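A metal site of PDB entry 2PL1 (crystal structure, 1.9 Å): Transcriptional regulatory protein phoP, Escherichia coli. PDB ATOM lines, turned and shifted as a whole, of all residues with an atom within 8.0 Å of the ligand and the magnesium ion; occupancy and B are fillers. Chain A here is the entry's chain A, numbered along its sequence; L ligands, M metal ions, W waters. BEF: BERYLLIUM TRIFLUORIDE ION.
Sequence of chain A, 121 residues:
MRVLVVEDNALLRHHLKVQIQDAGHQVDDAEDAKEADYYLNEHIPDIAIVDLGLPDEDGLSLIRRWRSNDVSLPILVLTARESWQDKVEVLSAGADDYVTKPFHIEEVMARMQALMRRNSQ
The side-chain hydroxyl of Thr 79 is in hydrogen-bond range of a fluorine (F2) of the ligand (2.5 Å).
The side-chain carboxylate (OD1) of Asp 51 is bound to a beryllium atom (BE) of the ligand (2.0 Å).
A fluorine (F2) of the ligand lies within hydrogen-bond range of the backbone NH of Leu 52, at 3.3 Å.
The side-chain amino group (NZ) of Lys 101 lies within hydrogen-bond range of a fluorine (F3) of the ligand, at 2.9 Å.
N of Ala 80 sits at hydrogen-bond distance from F3 of the ligand (2.9 Å).
N of Gly 53 is in hydrogen-bond range of F2 of the ligand, at 2.9 Å.
N of Thr 79 is in hydrogen-bond range of O of Val 99 (3.0 Å).
The side-chain amino group (NZ) of Lys 101 sits close to the side-chain carboxylate (OD1) of Asp 51, 3.5 Å away.
O of Val 6 lies within hydrogen-bond range of N of Asp 51 (2.9 Å).
The side-chain amino group of Lys 101 lies within salt-bridge range of the side-chain carboxylate of Glu 7, 2.8 Å away.
The side-chain hydroxyl (OG1) of Thr 79 lies within hydrogen-bond range of the backbone NH (N) of Arg 81.
N of Lys 101 sits at hydrogen-bond distance from O of Thr 79, 2.8 Å away.
The side-chain carboxylate (OE2) of Glu 7 lies within hydrogen-bond range of the backbone NH (N) of Asn 9 (2.9 Å).
The backbone carbonyl oxygen (O) of Leu 52 sits at hydrogen-bond distance from the backbone NH (N) of Gly 59 (2.8 Å).
Hydrophobic or aromatic side chains within 4 Å of the ligand: Leu 52 and Ala 80.
Six residues have an atom within 4 Å of the ligand: Asp 51, Leu 52, Gly 53, Thr 79, Ala 80 and Lys 101.
Glu 7 touches the magnesium ion.
Within 4 Å of the magnesium ion: Glu 7, Asp 8, Asp 51 and Gly 53.
The magnesium ion is bound by OD2 of Asp 51, at 2.2 Å.
The side-chain carboxylate (OD1) of Asp 8 binds the magnesium ion (2.2 Å).
Water W1 is bound to the magnesium ion, 2.3 Å away.
The magnesium ion is bound by O of Gly 53, 2.3 Å away.
Water W4 binds the magnesium ion, 2.3 Å away.
F1 of the ligand binds the magnesium ion, at 2.4 Å.
The magnesium ion has six donor atoms within binding distance.
Water W4 bridges OE2 of Glu 7 and NZ of Lys 101.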
ATOM      1  N   VAL A   6      20.440  18.800  20.233  1.00  0.00           N
ATOM      2  CA  VAL A   6      20.706  18.459  21.627  1.00  0.00           C
ATOM      3  C   VAL A   6      20.933  19.790  22.347  1.00  0.00           C
ATOM      4  O   VAL A   6      21.972  20.433  22.169  1.00  0.00           O
ATOM      5  CB  VAL A   6      21.980  17.586  21.759  1.00  0.00           C
ATOM      6  CG1 VAL A   6      22.134  17.096  23.196  1.00  0.00           C
ATOM      7  CG2 VAL A   6      21.910  16.404  20.796  1.00  0.00           C
ATOM      8  N   GLU A   7      19.953  20.181  23.156  1.00  0.00           N
ATOM      9  CA  GLU A   7      20.000  21.460  23.872  1.00  0.00           C
ATOM     10  C   GLU A   7      19.100  21.356  25.099  1.00  0.00           C
ATOM     11  O   GLU A   7      17.950  20.941  24.983  1.00  0.00           O
ATOM     12  CB  GLU A   7      19.485  22.556  22.925  1.00  0.00           C
ATOM     13  CG  GLU A   7      19.173  23.897  23.562  1.00  0.00           C
ATOM     14  CD  GLU A   7      20.379  24.547  24.200  1.00  0.00           C
ATOM     15  OE1 GLU A   7      21.399  24.731  23.489  1.00  0.00           O
ATOM     16  OE2 GLU A   7      20.305  24.880  25.398  1.00  0.00           O
ATOM     17  N   ASP A   8      19.596  21.734  26.282  1.00  0.00           N
ATOM     18  CA  ASP A   8      18.764  21.627  27.476  1.00  0.00           C
ATOM     19  C   ASP A   8      17.872  22.834  27.728  1.00  0.00           C
ATOM     20  O   ASP A   8      16.958  22.754  28.548  1.00  0.00           O
ATOM     21  CB  ASP A   8      19.609  21.314  28.720  1.00  0.00           C
ATOM     22  CG  ASP A   8      20.662  22.350  28.993  1.00  0.00           C
ATOM     23  OD1 ASP A   8      21.003  23.101  28.061  1.00  0.00           O
ATOM     24  OD2 ASP A   8      21.156  22.413  30.141  1.00  0.00           O
ATOM     25  N   ASN A   9      18.121  23.950  27.045  1.00  0.00           N
ATOM     26  CA  ASN A   9      17.272  25.132  27.190  1.00  0.00           C
ATOM     27  C   ASN A   9      16.047  24.828  26.330  1.00  0.00           C
ATOM     28  O   ASN A   9      16.104  24.914  25.104  1.00  0.00           O
ATOM     29  CB  ASN A   9      17.992  26.372  26.664  1.00  0.00           C
ATOM     30  CG  ASN A   9      17.159  27.648  26.811  1.00  0.00           C
ATOM     31  OD1 ASN A   9      16.025  27.716  26.343  1.00  0.00           O
ATOM     32  ND2 ASN A   9      17.742  28.645  27.460  1.00  0.00           N
ATOM     33  N   LEU A  12      14.884  27.456  23.593  1.00  0.00           N
ATOM     34  CA  LEU A  12      15.826  27.499  22.489  1.00  0.00           C
ATOM     35  C   LEU A  12      15.721  26.206  21.672  1.00  0.00           C
ATOM     36  O   LEU A  12      15.679  26.236  20.443  1.00  0.00           O
ATOM     37  CB  LEU A  12      17.261  27.644  23.023  1.00  0.00           C
ATOM     38  CG  LEU A  12      18.341  28.254  22.112  1.00  0.00           C
ATOM     39  CD1 LEU A  12      19.686  27.647  22.492  1.00  0.00           C
ATOM     40  CD2 LEU A  12      18.048  28.014  20.650  1.00  0.00           C
ATOM     41  N   GLU A  31      16.824  16.796  25.164  1.00  0.00           N
ATOM     42  CA  GLU A  31      17.168  17.766  26.196  1.00  0.00           C
ATOM     43  C   GLU A  31      18.410  17.460  27.025  1.00  0.00           C
ATOM     44  O   GLU A  31      18.823  18.280  27.850  1.00  0.00           O
ATOM     45  CB  GLU A  31      15.970  18.029  27.110  1.00  0.00           C
ATOM     46  CG  GLU A  31      15.403  16.806  27.802  1.00  0.00           C
ATOM     47  CD  GLU A  31      14.284  17.187  28.753  1.00  0.00           C
ATOM     48  OE1 GLU A  31      14.575  17.752  29.830  1.00  0.00           O
ATOM     49  OE2 GLU A  31      13.111  16.942  28.427  1.00  0.00           O
ATOM     50  N   VAL A  50      24.871  20.295  18.533  1.00  0.00           N
ATOM     51  CA  VAL A  50      25.096  19.944  19.924  1.00  0.00           C
ATOM     52  C   VAL A  50      25.518  21.073  20.863  1.00  0.00           C
ATOM     53  O   VAL A  50      26.467  21.811  20.602  1.00  0.00           O
ATOM     54  CB  VAL A  50      26.144  18.807  20.009  1.00  0.00           C
ATOM     55  CG1 VAL A  50      26.396  18.403  21.458  1.00  0.00           C
ATOM     56  CG2 VAL A  50      25.663  17.624  19.185  1.00  0.00           C
ATOM     57  N   ASP A  51      24.793  21.165  21.976  1.00  0.00           N
ATOM     58  CA  ASP A  51      25.037  22.145  23.014  1.00  0.00           C
ATOM     59  C   ASP A  51      26.059  21.490  23.955  1.00  0.00           C
ATOM     60  O   ASP A  51      26.023  20.276  24.135  1.00  0.00           O
ATOM     61  CB  ASP A  51      23.733  22.405  23.742  1.00  0.00           C
ATOM     62  CG  ASP A  51      23.887  23.343  24.882  1.00  0.00           C
ATOM     63  OD1 ASP A  51      24.734  24.253  24.798  1.00  0.00           O
ATOM     64  OD2 ASP A  51      23.139  23.178  25.857  1.00  0.00           O
ATOM     65  N   LEU A  52      26.947  22.277  24.561  1.00  0.00           N
ATOM     66  CA  LEU A  52      27.962  21.691  25.453  1.00  0.00           C
ATOM     67  C   LEU A  52      27.524  21.551  26.913  1.00  0.00           C
ATOM     68  O   LEU A  52      27.821  20.533  27.558  1.00  0.00           O
ATOM     69  CB  LEU A  52      29.265  22.493  25.369  1.00  0.00           C
ATOM     70  CG  LEU A  52      29.922  22.534  23.977  1.00  0.00           C
ATOM     71  CD1 LEU A  52      31.197  23.350  24.052  1.00  0.00           C
ATOM     72  CD2 LEU A  52      30.221  21.124  23.513  1.00  0.00           C
ATOM     73  N   GLY A  53      26.852  22.566  27.436  1.00  0.00           N
ATOM     74  CA  GLY A  53      26.404  22.518  28.814  1.00  0.00           C
ATOM     75  C   GLY A  53      25.126  21.727  28.952  1.00  0.00           C
ATOM     76  O   GLY A  53      24.049  22.220  28.623  1.00  0.00           O
ATOM     77  N   LEU A  54      25.225  20.489  29.430  1.00  0.00           N
ATOM     78  CA  LEU A  54      24.041  19.642  29.593  1.00  0.00           C
ATOM     79  C   LEU A  54      23.945  19.171  31.045  1.00  0.00           C
ATOM     80  O   LEU A  54      24.959  19.035  31.723  1.00  0.00           O
ATOM     81  CB  LEU A  54      24.111  18.459  28.627  1.00  0.00           C
ATOM     82  CG  LEU A  54      24.238  18.853  27.143  1.00  0.00           C
ATOM     83  CD1 LEU A  54      24.398  17.600  26.278  1.00  0.00           C
ATOM     84  CD2 LEU A  54      23.011  19.656  26.703  1.00  0.00           C
ATOM     85  N   PRO A  55      22.718  18.915  31.533  1.00  0.00           N
ATOM     86  CA  PRO A  55      22.454  18.465  32.907  1.00  0.00           C
ATOM     87  C   PRO A  55      23.328  17.355  33.454  1.00  0.00           C
ATOM     88  O   PRO A  55      23.713  17.386  34.617  1.00  0.00           O
ATOM     89  CB  PRO A  55      20.967  18.108  32.878  1.00  0.00           C
ATOM     90  CG  PRO A  55      20.689  17.809  31.447  1.00  0.00           C
ATOM     91  CD  PRO A  55      21.479  18.874  30.733  1.00  0.00           C
ATOM     92  N   GLY A  59      28.365  18.056  26.482  1.00  0.00           N
ATOM     93  CA  GLY A  59      28.494  17.884  25.047  1.00  0.00           C
ATOM     94  C   GLY A  59      29.826  17.358  24.548  1.00  0.00           C
ATOM     95  O   GLY A  59      29.876  16.549  23.621  1.00  0.00           O
ATOM     96  N   VAL A  77      28.601  22.389  16.868  1.00  0.00           N
ATOM     97  CA  VAL A  77      28.382  22.765  18.257  1.00  0.00           C
ATOM     98  C   VAL A  77      27.901  24.206  18.347  1.00  0.00           C
ATOM     99  O   VAL A  77      28.419  25.092  17.672  1.00  0.00           O
ATOM    100  CB  VAL A  77      29.680  22.583  19.080  1.00  0.00           C
ATOM    101  CG1 VAL A  77      29.532  23.213  20.466  1.00  0.00           C
ATOM    102  CG2 VAL A  77      29.999  21.101  19.198  1.00  0.00           C
ATOM    103  N   LEU A  78      26.877  24.431  19.168  1.00  0.00           N
ATOM    104  CA  LEU A  78      26.289  25.753  19.383  1.00  0.00           C
ATOM    105  C   LEU A  78      26.259  25.880  20.898  1.00  0.00           C
ATOM    106  O   LEU A  78      25.462  25.232  21.571  1.00  0.00           O
ATOM    107  CB  LEU A  78      24.866  25.789  18.813  1.00  0.00           C
ATOM    108  CG  LEU A  78      24.082  27.103  18.957  1.00  0.00           C
ATOM    109  CD1 LEU A  78      24.866  28.260  18.319  1.00  0.00           C
ATOM    110  CD2 LEU A  78      22.717  26.942  18.283  1.00  0.00           C
ATOM    111  N   THR A  79      27.127  26.746  21.427  1.00  0.00           N
ATOM    112  CA  THR A  79      27.282  26.855  22.873  1.00  0.00           C
ATOM    113  C   THR A  79      27.604  28.239  23.425  1.00  0.00           C
ATOM    114  O   THR A  79      28.058  29.127  22.697  1.00  0.00           O
ATOM    115  CB  THR A  79      28.421  25.905  23.283  1.00  0.00           C
ATOM    116  OG1 THR A  79      28.749  26.090  24.667  1.00  0.00           O
ATOM    117  CG2 THR A  79      29.669  26.200  22.455  1.00  0.00           C
ATOM    118  N   ALA A  80      27.384  28.411  24.723  1.00  0.00           N
ATOM    119  CA  ALA A  80      27.679  29.673  25.401  1.00  0.00           C
ATOM    120  C   ALA A  80      29.163  29.717  25.764  1.00  0.00           C
ATOM    121  O   ALA A  80      29.682  30.760  26.134  1.00  0.00           O
ATOM    122  CB  ALA A  80      26.824  29.822  26.664  1.00  0.00           C
ATOM    123  N   ARG A  81      29.844  28.577  25.652  1.00  0.00           N
ATOM    124  CA  ARG A  81      31.276  28.528  25.957  1.00  0.00           C
ATOM    125  C   ARG A  81      32.002  29.220  24.798  1.00  0.00           C
ATOM    126  O   ARG A  81      32.037  28.707  23.686  1.00  0.00           O
ATOM    127  CB  ARG A  81      31.745  27.078  26.093  1.00  0.00           C
ATOM    128  CG  ARG A  81      31.070  26.328  27.231  1.00  0.00           C
ATOM    129  CD  ARG A  81      32.101  25.670  28.157  1.00  0.00           C
ATOM    130  NE  ARG A  81      32.602  24.397  27.644  1.00  0.00           N
ATOM    131  CZ  ARG A  81      32.024  23.218  27.845  1.00  0.00           C
ATOM    132  NH1 ARG A  81      30.911  23.140  28.564  1.00  0.00           N
ATOM    133  NH2 ARG A  81      32.550  22.113  27.335  1.00  0.00           N
ATOM    134  N   GLU A  82      32.580  30.380  25.084  1.00  0.00           N
ATOM    135  CA  GLU A  82      33.252  31.179  24.052  1.00  0.00           C
ATOM    136  C   GLU A  82      34.767  31.128  23.897  1.00  0.00           C
ATOM    137  O   GLU A  82      35.281  31.567  22.866  1.00  0.00           O
ATOM    138  CB  GLU A  82      32.857  32.652  24.217  1.00  0.00           C
ATOM    139  CG  GLU A  82      31.386  32.958  24.032  1.00  0.00           C
ATOM    140  CD  GLU A  82      31.095  34.446  24.135  1.00  0.00           C
ATOM    141  OE1 GLU A  82      31.227  35.023  25.236  1.00  0.00           O
ATOM    142  OE2 GLU A  82      30.730  35.043  23.098  1.00  0.00           O
ATOM    143  N   TYR A  98      31.872  25.107  15.228  1.00  0.00           N
ATOM    144  CA  TYR A  98      31.626  25.574  16.573  1.00  0.00           C
ATOM    145  C   TYR A  98      31.140  27.025  16.488  1.00  0.00           C
ATOM    146  O   TYR A  98      31.854  27.887  15.983  1.00  0.00           O
ATOM    147  CB  TYR A  98      32.897  25.467  17.341  1.00  0.00           C
ATOM    148  CG  TYR A  98      32.894  25.697  18.863  1.00  0.00           C
ATOM    149  CD1 TYR A  98      32.468  26.900  19.405  1.00  0.00           C
ATOM    150  CD2 TYR A  98      33.288  24.679  19.718  1.00  0.00           C
ATOM    151  CE1 TYR A  98      32.504  27.114  20.790  1.00  0.00           C
ATOM    152  CE2 TYR A  98      33.325  24.871  21.100  1.00  0.00           C
ATOM    153  CZ  TYR A  98      32.937  26.095  21.628  1.00  0.00           C
ATOM    154  OH  TYR A  98      33.002  26.291  22.986  1.00  0.00           O
ATOM    155  N   VAL A  99      29.917  27.255  16.956  1.00  0.00           N
ATOM    156  CA  VAL A  99      29.311  28.585  16.946  1.00  0.00           C
ATOM    157  C   VAL A  99      28.963  28.984  18.377  1.00  0.00           C
ATOM    158  O   VAL A  99      28.471  28.161  19.153  1.00  0.00           O
ATOM    159  CB  VAL A  99      28.034  28.602  16.080  1.00  0.00           C
ATOM    160  CG1 VAL A  99      27.389  29.994  16.105  1.00  0.00           C
ATOM    161  CG2 VAL A  99      28.373  28.197  14.659  1.00  0.00           C
ATOM    162  N   THR A 100      29.213  30.235  18.735  1.00  0.00           N
ATOM    163  CA  THR A 100      28.927  30.701  20.084  1.00  0.00           C
ATOM    164  C   THR A 100      27.578  31.407  20.198  1.00  0.00           C
ATOM    165  O   THR A 100      27.069  31.965  19.222  1.00  0.00           O
ATOM    166  CB  THR A 100      30.019  31.686  20.573  1.00  0.00           C
ATOM    167  OG1 THR A 100      30.139  32.765  19.646  1.00  0.00           O
ATOM    168  CG2 THR A 100      31.357  30.979  20.691  1.00  0.00           C
ATOM    169  N   LYS A 101      27.005  31.371  21.402  1.00  0.00           N
ATOM    170  CA  LYS A 101      25.752  32.055  21.686  1.00  0.00           C
ATOM    171  C   LYS A 101      26.165  33.371  22.352  1.00  0.00           C
ATOM    172  O   LYS A 101      27.150  33.383  23.098  1.00  0.00           O
ATOM    173  CB  LYS A 101      24.906  31.257  22.687  1.00  0.00           C
ATOM    174  CG  LYS A 101      24.484  29.854  22.254  1.00  0.00           C
ATOM    175  CD  LYS A 101      23.789  29.150  23.414  1.00  0.00           C
ATOM    176  CE  LYS A 101      23.333  27.750  23.048  1.00  0.00           C
ATOM    177  NZ  LYS A 101      22.771  27.052  24.246  1.00  0.00           N
HETATM  178 BE   BEF L   1      25.493  25.417  26.188  1.00  0.00          BE
HETATM  179  F1  BEF L   1      25.022  25.190  27.579  1.00  0.00           F
HETATM  180  F2  BEF L   1      26.970  25.148  26.105  1.00  0.00           F
HETATM  181  F3  BEF L   1      25.182  26.814  25.768  1.00  0.00           F
HETATM  182 MG    MG M   1      22.962  24.062  27.847  1.00  0.00          MG
HETATM  183  O   HOH W   1      23.141  24.845  29.973  1.00  0.00           O
HETATM  184  O   HOH W   2      25.281  26.245  30.298  1.00  0.00           O
HETATM  185  O   HOH W   3      23.797  28.543  27.806  1.00  0.00           O
HETATM  186  O   HOH W   4      21.950  25.887  26.880  1.00  0.00           O
